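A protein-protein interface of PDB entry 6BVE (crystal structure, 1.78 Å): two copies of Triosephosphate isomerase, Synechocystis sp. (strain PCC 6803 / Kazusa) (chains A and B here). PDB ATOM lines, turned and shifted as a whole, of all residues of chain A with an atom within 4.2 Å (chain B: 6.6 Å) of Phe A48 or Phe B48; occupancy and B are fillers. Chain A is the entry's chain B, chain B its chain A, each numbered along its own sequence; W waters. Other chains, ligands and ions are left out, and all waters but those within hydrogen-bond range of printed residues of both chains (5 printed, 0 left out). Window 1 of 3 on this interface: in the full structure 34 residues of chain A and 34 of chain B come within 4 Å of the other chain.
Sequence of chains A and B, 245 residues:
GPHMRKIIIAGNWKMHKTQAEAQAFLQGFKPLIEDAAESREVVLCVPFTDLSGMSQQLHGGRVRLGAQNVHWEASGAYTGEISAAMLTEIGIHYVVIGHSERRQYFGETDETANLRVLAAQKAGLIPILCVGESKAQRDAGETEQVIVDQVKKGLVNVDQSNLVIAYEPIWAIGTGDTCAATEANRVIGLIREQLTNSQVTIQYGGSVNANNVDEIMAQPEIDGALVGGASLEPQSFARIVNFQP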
ATOM      1  N   VAL A  46     -16.709 -26.817  -5.913  1.00  0.00           N
ATOM      2  CA  VAL A  46     -17.931 -26.371  -6.578  1.00  0.00           C
ATOM      3  C   VAL A  46     -17.539 -25.507  -7.766  1.00  0.00           C
ATOM      4  O   VAL A  46     -16.389 -25.033  -7.857  1.00  0.00           O
ATOM      5  CB  VAL A  46     -18.855 -25.596  -5.608  1.00  0.00           C
ATOM      6  CG1 VAL A  46     -19.132 -26.433  -4.368  1.00  0.00           C
ATOM      7  CG2 VAL A  46     -18.184 -24.295  -5.190  1.00  0.00           C
ATOM      8  N   PRO A  47     -18.478 -25.263  -8.689  1.00  0.00           N
ATOM      9  CA  PRO A  47     -18.196 -24.379  -9.829  1.00  0.00           C
ATOM     10  C   PRO A  47     -17.806 -22.984  -9.371  1.00  0.00           C
ATOM     11  O   PRO A  47     -18.233 -22.523  -8.313  1.00  0.00           O
ATOM     12  CB  PRO A  47     -19.519 -24.351 -10.598  1.00  0.00           C
ATOM     13  CG  PRO A  47     -20.177 -25.701 -10.253  1.00  0.00           C
ATOM     14  CD  PRO A  47     -19.769 -25.983  -8.836  1.00  0.00           C
ATOM     15  N   PHE A  48     -16.989 -22.307 -10.194  1.00  0.00           N
ATOM     16  CA  PHE A  48     -16.539 -20.957  -9.858  1.00  0.00           C
ATOM     17  C   PHE A  48     -17.698 -20.052  -9.460  1.00  0.00           C
ATOM     18  O   PHE A  48     -17.582 -19.245  -8.534  1.00  0.00           O
ATOM     19  CB  PHE A  48     -15.825 -20.313 -11.050  1.00  0.00           C
ATOM     20  CG  PHE A  48     -14.537 -20.978 -11.429  1.00  0.00           C
ATOM     21  CD1 PHE A  48     -13.512 -21.113 -10.501  1.00  0.00           C
ATOM     22  CD2 PHE A  48     -14.336 -21.426 -12.710  1.00  0.00           C
ATOM     23  CE1 PHE A  48     -12.314 -21.717 -10.851  1.00  0.00           C
ATOM     24  CE2 PHE A  48     -13.132 -22.020 -13.072  1.00  0.00           C
ATOM     25  CZ  PHE A  48     -12.132 -22.167 -12.150  1.00  0.00           C
ATOM     26  N   THR A  49     -18.800 -20.130 -10.201  1.00  0.00           N
ATOM     27  CA  THR A  49     -19.929 -19.222 -10.027  1.00  0.00           C
ATOM     28  C   THR A  49     -20.735 -19.496  -8.758  1.00  0.00           C
ATOM     29  O   THR A  49     -21.611 -18.690  -8.409  1.00  0.00           O
ATOM     30  CB  THR A  49     -20.812 -19.313 -11.268  1.00  0.00           C
ATOM     31  OG1 THR A  49     -21.004 -20.687 -11.602  1.00  0.00           O
ATOM     32  CG2 THR A  49     -20.123 -18.626 -12.451  1.00  0.00           C
ATOM     33  N   ASP A  50     -20.453 -20.590  -8.048  1.00  0.00           N
ATOM     34  CA  ASP A  50     -21.100 -20.891  -6.776  1.00  0.00           C
ATOM     35  C   ASP A  50     -20.259 -20.508  -5.564  1.00  0.00           C
ATOM     36  O   ASP A  50     -20.768 -20.561  -4.439  1.00  0.00           O
ATOM     37  CB  ASP A  50     -21.406 -22.389  -6.658  1.00  0.00           C
ATOM     38  CG  ASP A  50     -22.480 -22.866  -7.636  1.00  0.00           C
ATOM     39  OD1 ASP A  50     -23.297 -22.040  -8.081  1.00  0.00           O
ATOM     40  OD2 ASP A  50     -22.497 -24.074  -7.951  1.00  0.00           O
ATOM     41  N   LEU A  51     -18.976 -20.189  -5.751  1.00  0.00           N
ATOM     42  CA  LEU A  51     -18.071 -20.066  -4.609  1.00  0.00           C
ATOM     43  C   LEU A  51     -18.478 -18.934  -3.672  1.00  0.00           C
ATOM     44  O   LEU A  51     -18.585 -19.130  -2.458  1.00  0.00           O
ATOM     45  CB  LEU A  51     -16.643 -19.828  -5.085  1.00  0.00           C
ATOM     46  CG  LEU A  51     -15.913 -21.005  -5.750  1.00  0.00           C
ATOM     47  CD1 LEU A  51     -14.690 -20.441  -6.476  1.00  0.00           C
ATOM     48  CD2 LEU A  51     -15.513 -22.053  -4.714  1.00  0.00           C
ATOM     49  N   ALA A  67     -12.330 -24.730  -5.129  1.00  0.00           N
ATOM     50  CA  ALA A  67     -12.570 -24.550  -6.550  1.00  0.00           C
ATOM     51  C   ALA A  67     -12.118 -25.815  -7.277  1.00  0.00           C
ATOM     52  O   ALA A  67     -11.449 -26.685  -6.707  1.00  0.00           O
ATOM     53  CB  ALA A  67     -11.837 -23.319  -7.083  1.00  0.00           C
ATOM     54  N   ASN A  69     -10.399 -25.704 -10.276  1.00  0.00           N
ATOM     55  CA  ASN A  69      -9.236 -25.404 -11.097  1.00  0.00           C
ATOM     56  C   ASN A  69      -8.709 -24.054 -10.634  1.00  0.00           C
ATOM     57  O   ASN A  69      -9.425 -23.285  -9.988  1.00  0.00           O
ATOM     58  CB  ASN A  69      -9.595 -25.363 -12.582  1.00  0.00           C
ATOM     59  CG  ASN A  69      -8.387 -25.545 -13.498  1.00  0.00           C
ATOM     60  OD1 ASN A  69      -7.275 -25.850 -13.048  1.00  0.00           O
ATOM     61  ND2 ASN A  69      -8.603 -25.337 -14.793  1.00  0.00           N
ATOM     62  N   GLY A  80     -10.666 -17.126 -20.072  1.00  0.00           N
ATOM     63  CA  GLY A  80     -11.419 -18.187 -19.434  1.00  0.00           C
ATOM     64  C   GLY A  80     -10.856 -18.709 -18.117  1.00  0.00           C
ATOM     65  O   GLY A  80     -11.588 -19.390 -17.384  1.00  0.00           O
ATOM     66  N   ILE A  82      -9.061 -18.683 -14.204  1.00  0.00           N
ATOM     67  CA  ILE A  82      -9.243 -18.030 -12.913  1.00  0.00           C
ATOM     68  C   ILE A  82      -7.926 -18.095 -12.152  1.00  0.00           C
ATOM     69  O   ILE A  82      -7.283 -19.154 -12.099  1.00  0.00           O
ATOM     70  CB  ILE A  82     -10.365 -18.721 -12.116  1.00  0.00           C
ATOM     71  CG1 ILE A  82     -11.699 -18.632 -12.871  1.00  0.00           C
ATOM     72  CG2 ILE A  82     -10.454 -18.182 -10.725  1.00  0.00           C
ATOM     73  CD1 ILE A  82     -12.209 -17.201 -13.146  1.00  0.00           C
ATOM     74  N   VAL B  46     -15.562 -10.844 -18.565  1.00  0.00           N
ATOM     75  CA  VAL B  46     -14.820 -10.790 -17.310  1.00  0.00           C
ATOM     76  C   VAL B  46     -14.697 -12.200 -16.746  1.00  0.00           C
ATOM     77  O   VAL B  46     -15.431 -13.118 -17.149  1.00  0.00           O
ATOM     78  CB  VAL B  46     -15.505  -9.840 -16.297  1.00  0.00           C
ATOM     79  CG1 VAL B  46     -15.734  -8.439 -16.920  1.00  0.00           C
ATOM     80  CG2 VAL B  46     -16.812 -10.431 -15.813  1.00  0.00           C
ATOM     81  N   PRO B  47     -13.776 -12.402 -15.807  1.00  0.00           N
ATOM     82  CA  PRO B  47     -13.623 -13.731 -15.192  1.00  0.00           C
ATOM     83  C   PRO B  47     -14.905 -14.198 -14.519  1.00  0.00           C
ATOM     84  O   PRO B  47     -15.699 -13.395 -14.032  1.00  0.00           O
ATOM     85  CB  PRO B  47     -12.506 -13.518 -14.166  1.00  0.00           C
ATOM     86  CG  PRO B  47     -11.682 -12.407 -14.761  1.00  0.00           C
ATOM     87  CD  PRO B  47     -12.719 -11.469 -15.361  1.00  0.00           C
ATOM     88  N   PHE B  48     -15.098 -15.530 -14.493  1.00  0.00           N
ATOM     89  CA  PHE B  48     -16.315 -16.107 -13.904  1.00  0.00           C
ATOM     90  C   PHE B  48     -16.602 -15.527 -12.525  1.00  0.00           C
ATOM     91  O   PHE B  48     -17.764 -15.281 -12.164  1.00  0.00           O
ATOM     92  CB  PHE B  48     -16.170 -17.623 -13.760  1.00  0.00           C
ATOM     93  CG  PHE B  48     -16.142 -18.371 -15.051  1.00  0.00           C
ATOM     94  CD1 PHE B  48     -17.179 -18.252 -15.970  1.00  0.00           C
ATOM     95  CD2 PHE B  48     -15.080 -19.217 -15.342  1.00  0.00           C
ATOM     96  CE1 PHE B  48     -17.134 -18.980 -17.178  1.00  0.00           C
ATOM     97  CE2 PHE B  48     -15.037 -19.929 -16.535  1.00  0.00           C
ATOM     98  CZ  PHE B  48     -16.061 -19.804 -17.454  1.00  0.00           C
ATOM     99  N   THR B  49     -15.550 -15.337 -11.726  1.00  0.00           N
ATOM    100  CA  THR B  49     -15.719 -14.937 -10.333  1.00  0.00           C
ATOM    101  C   THR B  49     -16.103 -13.470 -10.171  1.00  0.00           C
ATOM    102  O   THR B  49     -16.435 -13.060  -9.054  1.00  0.00           O
ATOM    103  CB  THR B  49     -14.429 -15.246  -9.568  1.00  0.00           C
ATOM    104  OG1 THR B  49     -13.294 -14.768 -10.316  1.00  0.00           O
ATOM    105  CG2 THR B  49     -14.301 -16.771  -9.398  1.00  0.00           C
ATOM    106  N   ASP B  50     -16.072 -12.693 -11.252  1.00  0.00           N
ATOM    107  CA  ASP B  50     -16.483 -11.295 -11.259  1.00  0.00           C
ATOM    108  C   ASP B  50     -17.916 -11.094 -11.746  1.00  0.00           C
ATOM    109  O   ASP B  50     -18.453  -9.998 -11.601  1.00  0.00           O
ATOM    110  CB  ASP B  50     -15.539 -10.464 -12.161  1.00  0.00           C
ATOM    111  CG  ASP B  50     -14.156 -10.289 -11.577  1.00  0.00           C
ATOM    112  OD1 ASP B  50     -13.990 -10.465 -10.361  1.00  0.00           O
ATOM    113  OD2 ASP B  50     -13.226  -9.945 -12.346  1.00  0.00           O
ATOM    114  N   LEU B  51     -18.543 -12.120 -12.327  1.00  0.00           N
ATOM    115  CA  LEU B  51     -19.814 -11.919 -13.024  1.00  0.00           C
ATOM    116  C   LEU B  51     -20.923 -11.442 -12.090  1.00  0.00           C
ATOM    117  O   LEU B  51     -21.608 -10.457 -12.381  1.00  0.00           O
ATOM    118  CB  LEU B  51     -20.244 -13.215 -13.709  1.00  0.00           C
ATOM    119  CG  LEU B  51     -19.352 -13.673 -14.872  1.00  0.00           C
ATOM    120  CD1 LEU B  51     -19.734 -15.102 -15.330  1.00  0.00           C
ATOM    121  CD2 LEU B  51     -19.470 -12.699 -16.051  1.00  0.00           C
ATOM    122  N   SER B  52     -21.137 -12.151 -10.977  1.00  0.00           N
ATOM    123  CA  SER B  52     -22.276 -11.848 -10.110  1.00  0.00           C
ATOM    124  C   SER B  52     -22.150 -10.459  -9.501  1.00  0.00           C
ATOM    125  O   SER B  52     -23.100  -9.666  -9.527  1.00  0.00           O
ATOM    126  CB  SER B  52     -22.394 -12.904  -9.008  1.00  0.00           C
ATOM    127  OG  SER B  52     -22.866 -14.128  -9.527  1.00  0.00           O
ATOM    128  N   ALA B  67     -19.239 -13.613 -20.268  1.00  0.00           N
ATOM    129  CA  ALA B  67     -18.297 -14.599 -19.748  1.00  0.00           C
ATOM    130  C   ALA B  67     -17.212 -14.855 -20.792  1.00  0.00           C
ATOM    131  O   ALA B  67     -17.350 -14.502 -21.958  1.00  0.00           O
ATOM    132  CB  ALA B  67     -19.011 -15.915 -19.407  1.00  0.00           C
ATOM    133  N   GLN B  68     -16.120 -15.479 -20.359  1.00  0.00           N
ATOM    134  CA  GLN B  68     -15.013 -15.753 -21.262  1.00  0.00           C
ATOM    135  C   GLN B  68     -14.993 -17.193 -21.755  1.00  0.00           C
ATOM    136  O   GLN B  68     -14.071 -17.567 -22.493  1.00  0.00           O
ATOM    137  CB  GLN B  68     -13.689 -15.421 -20.575  1.00  0.00           C
ATOM    138  CG  GLN B  68     -13.488 -13.922 -20.375  1.00  0.00           C
ATOM    139  CD  GLN B  68     -12.229 -13.628 -19.587  1.00  0.00           C
ATOM    140  OE1 GLN B  68     -11.357 -14.496 -19.435  1.00  0.00           O
ATOM    141  NE2 GLN B  68     -12.135 -12.418 -19.048  1.00  0.00           N
ATOM    142  N   ASN B  69     -15.986 -17.997 -21.368  1.00  0.00           N
ATOM    143  CA  ASN B  69     -16.130 -19.375 -21.818  1.00  0.00           C
ATOM    144  C   ASN B  69     -17.467 -19.894 -21.315  1.00  0.00           C
ATOM    145  O   ASN B  69     -18.059 -19.339 -20.383  1.00  0.00           O
ATOM    146  CB  ASN B  69     -14.991 -20.251 -21.295  1.00  0.00           C
ATOM    147  CG  ASN B  69     -14.788 -21.508 -22.114  1.00  0.00           C
ATOM    148  OD1 ASN B  69     -15.363 -21.666 -23.181  1.00  0.00           O
ATOM    149  ND2 ASN B  69     -13.955 -22.404 -21.616  1.00  0.00           N
ATOM    150  N   VAL B  70     -17.932 -20.965 -21.949  1.00  0.00           N
ATOM    151  CA  VAL B  70     -19.082 -21.735 -21.472  1.00  0.00           C
ATOM    152  C   VAL B  70     -18.908 -23.123 -22.061  1.00  0.00           C
ATOM    153  O   VAL B  70     -18.369 -23.273 -23.160  1.00  0.00           O
ATOM    154  CB  VAL B  70     -20.432 -21.093 -21.887  1.00  0.00           C
ATOM    155  CG1 VAL B  70     -20.646 -21.152 -23.405  1.00  0.00           C
ATOM    156  CG2 VAL B  70     -21.601 -21.766 -21.155  1.00  0.00           C
ATOM    157  N   GLY B  80     -14.219 -28.207 -13.527  1.00  0.00           N
ATOM    158  CA  GLY B  80     -13.680 -26.907 -13.845  1.00  0.00           C
ATOM    159  C   GLY B  80     -14.488 -26.082 -14.827  1.00  0.00           C
ATOM    160  O   GLY B  80     -14.215 -24.883 -14.962  1.00  0.00           O
ATOM    161  N   GLU B  81     -15.460 -26.674 -15.516  1.00  0.00           N
ATOM    162  CA  GLU B  81     -16.213 -25.995 -16.560  1.00  0.00           C
ATOM    163  C   GLU B  81     -17.478 -25.364 -15.991  1.00  0.00           C
ATOM    164  O   GLU B  81     -18.010 -25.811 -14.976  1.00  0.00           O
ATOM    165  CB  GLU B  81     -16.594 -26.969 -17.675  1.00  0.00           C
ATOM    166  CG  GLU B  81     -15.390 -27.470 -18.463  1.00  0.00           C
ATOM    167  CD  GLU B  81     -14.736 -26.352 -19.254  1.00  0.00           C
ATOM    168  OE1 GLU B  81     -15.386 -25.832 -20.191  1.00  0.00           O
ATOM    169  OE2 GLU B  81     -13.577 -25.990 -18.938  1.00  0.00           O
ATOM    170  N   ILE B  82     -17.974 -24.345 -16.694  1.00  0.00           N
ATOM    171  CA  ILE B  82     -19.162 -23.583 -16.302  1.00  0.00           C
ATOM    172  C   ILE B  82     -20.236 -23.782 -17.364  1.00  0.00           C
ATOM    173  O   ILE B  82     -19.951 -23.687 -18.563  1.00  0.00           O
ATOM    174  CB  ILE B  82     -18.828 -22.079 -16.149  1.00  0.00           C
ATOM    175  CG1 ILE B  82     -17.741 -21.858 -15.083  1.00  0.00           C
ATOM    176  CG2 ILE B  82     -20.092 -21.258 -15.861  1.00  0.00           C
ATOM    177  CD1 ILE B  82     -18.132 -22.341 -13.670  1.00  0.00           C
ATOM    178  N   MET B  86     -25.572 -21.865 -15.429  1.00  0.00           N
ATOM    179  CA  MET B  86     -24.872 -21.070 -14.423  1.00  0.00           C
ATOM    180  C   MET B  86     -24.732 -19.622 -14.859  1.00  0.00           C
ATOM    181  O   MET B  86     -24.795 -18.706 -14.023  1.00  0.00           O
ATOM    182  CB  MET B  86     -23.502 -21.678 -14.145  1.00  0.00           C
ATOM    183  CG  MET B  86     -23.612 -23.070 -13.512  1.00  0.00           C
ATOM    184  SD  MET B  86     -22.019 -23.913 -13.471  1.00  0.00           S
ATOM    185  CE  MET B  86     -22.562 -25.577 -13.057  1.00  0.00           C
ATOM    186  N   LEU B  87     -24.561 -19.393 -16.161  1.00  0.00           N
ATOM    187  CA  LEU B  87     -24.405 -18.026 -16.648  1.00  0.00           C
ATOM    188  C   LEU B  87     -25.739 -17.295 -16.753  1.00  0.00           C
ATOM    189  O   LEU B  87     -25.831 -16.110 -16.398  1.00  0.00           O
ATOM    190  CB  LEU B  87     -23.698 -18.045 -18.005  1.00  0.00           C
ATOM    191  CG  LEU B  87     -22.258 -18.574 -17.991  1.00  0.00           C
ATOM    192  CD1 LEU B  87     -21.615 -18.469 -19.379  1.00  0.00           C
ATOM    193  CD2 LEU B  87     -21.407 -17.823 -16.957  1.00  0.00           C
ATOM    194  N   ILE B  90     -27.165 -15.685 -13.602  1.00  0.00           N
ATOM    195  CA  ILE B  90     -26.612 -14.378 -13.261  1.00  0.00           C
ATOM    196  C   ILE B  90     -27.227 -13.285 -14.121  1.00  0.00           C
ATOM    197  O   ILE B  90     -27.261 -12.122 -13.708  1.00  0.00           O
ATOM    198  CB  ILE B  90     -25.076 -14.386 -13.406  1.00  0.00           C
ATOM    199  CG1 ILE B  90     -24.493 -15.556 -12.601  1.00  0.00           C
ATOM    200  CG2 ILE B  90     -24.445 -13.022 -12.998  1.00  0.00           C
ATOM    201  CD1 ILE B  90     -22.984 -15.815 -12.831  1.00  0.00           C
ATOM    202  N   VAL B  95     -21.034 -14.337 -24.305  1.00  0.00           N
ATOM    203  CA  VAL B  95     -19.947 -15.234 -23.925  1.00  0.00           C
ATOM    204  C   VAL B  95     -18.955 -15.319 -25.081  1.00  0.00           C
ATOM    205  O   VAL B  95     -19.337 -15.542 -26.236  1.00  0.00           O
ATOM    206  CB  VAL B  95     -20.451 -16.636 -23.505  1.00  0.00           C
ATOM    207  CG1 VAL B  95     -21.334 -17.233 -24.550  1.00  0.00           C
ATOM    208  CG2 VAL B  95     -19.262 -17.551 -23.199  1.00  0.00           C
HETATM  209  O   HOH W   1     -15.400 -24.290 -11.940  1.00  0.00           O
HETATM  210  O   HOH W   2     -13.430 -16.881 -16.631  1.00  0.00           O
HETATM  211  O   HOH W   3     -12.905 -21.690 -18.765  1.00  0.00           O
HETATM  212  O   HOH W   4     -11.361 -24.095 -15.258  1.00  0.00           O
HETATM  213  O   HOH W   5     -21.432 -16.241  -9.434  1.00  0.00           O
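Printed residues of chain A that touch a printed residue of chain B: Pro A47, Phe A48, Thr A49, Gly A80 and Ile A82.
Hydrophobic or aromatic side chains of chain A within 4 Å of the printed part of chain B: Pro A47, Phe A48 and Ile A82.
Along chain A the printed residues that touch a printed residue of chain B span positions 47 to 82.
Among the printed residues, 12 pairs touch across the chains.
Among the printed residues, no Asp or Glu carboxylate lies within 4 Å of a Lys or Arg side-chain nitrogen of the other chain.
The backbone NH of Gly A80 is in hydrogen-bond range of the side-chain amide oxygen of Gln B68.
Water W5 bridges the side-chain hydroxyl (OG) of Ser B52 and the backbone carbonyl oxygen (O) of Thr A49.
Water W4 lies within hydrogen-bond range of O of Gly B80 (3.0 Å) and ND2 of Asn A69 (3.1 Å).
Water W3 lies within hydrogen-bond range of the backbone carbonyl oxygen (O) of Gly A80 (3.0 Å) and the side-chain amide nitrogen (ND2) of Asn B69 (3.1 Å).
Water W2 bridges the backbone NH of Phe B48 and the backbone carbonyl oxygen of Gly A80.
Water W1 bridges N of Phe A48 and O of Gly B80.
Pro A47 touches Ile B82, and with the chains exchanged Ile A82 touches Pro B47.
Phe B48 touches its own counterpart, Phe A48.
Phe A48 touches Ile B82, and with the chains exchanged Ile A82 touches Phe B48.
Thr A49 touches Ile B82, and with the chains exchanged Ile A82 touches Thr B49.
Of the 12 pairs that touch across the chains among the printed residues, 9 have their exchanged pair printed and touching as well.
Among the printed residues, merely in contact across the chains: Phe A48 with Phe B48 (3.5 Å), Gly A80 with Phe B48 (3.6 Å), Phe A48 with Gly B80 (3.6 Å), Ile A82 with Phe B48 (3.6 Å), Phe A48 with Ile B82 (3.7 Å), Pro A47 with Met B86 (3.7 Å), Thr A49 with Met B86 (3.7 Å), Ile A82 with Pro B47 (3.8 Å), Ile A82 with Thr B49 (3.9 Å), Thr A49 with Ile B82 (3.9 Å) and Pro A47 with Ile B82 (3.9 Å).
Of chain B, only Phe B48 (3.5 Å), Gly B80 (3.6 Å) and Ile B82 (3.7 Å) come within 4 Å of Phe A48.
Of the printed residues of chain A, Met B86 touches Pro A47 (3.7 Å) and Thr A49 (3.7 Å).
Printed residues of chain B within 4 Å of Pro A47: Ile B82 and Met B86.
Of the printed residues of chain A, Gly B80 touches Phe A48.
Printed residues of chain B within 4 Å of Thr A49: Ile B82 and Met B86.
Ala A67 touches none of the printed residues of chain B.
Val A46 touches none of the printed residues of chain B.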
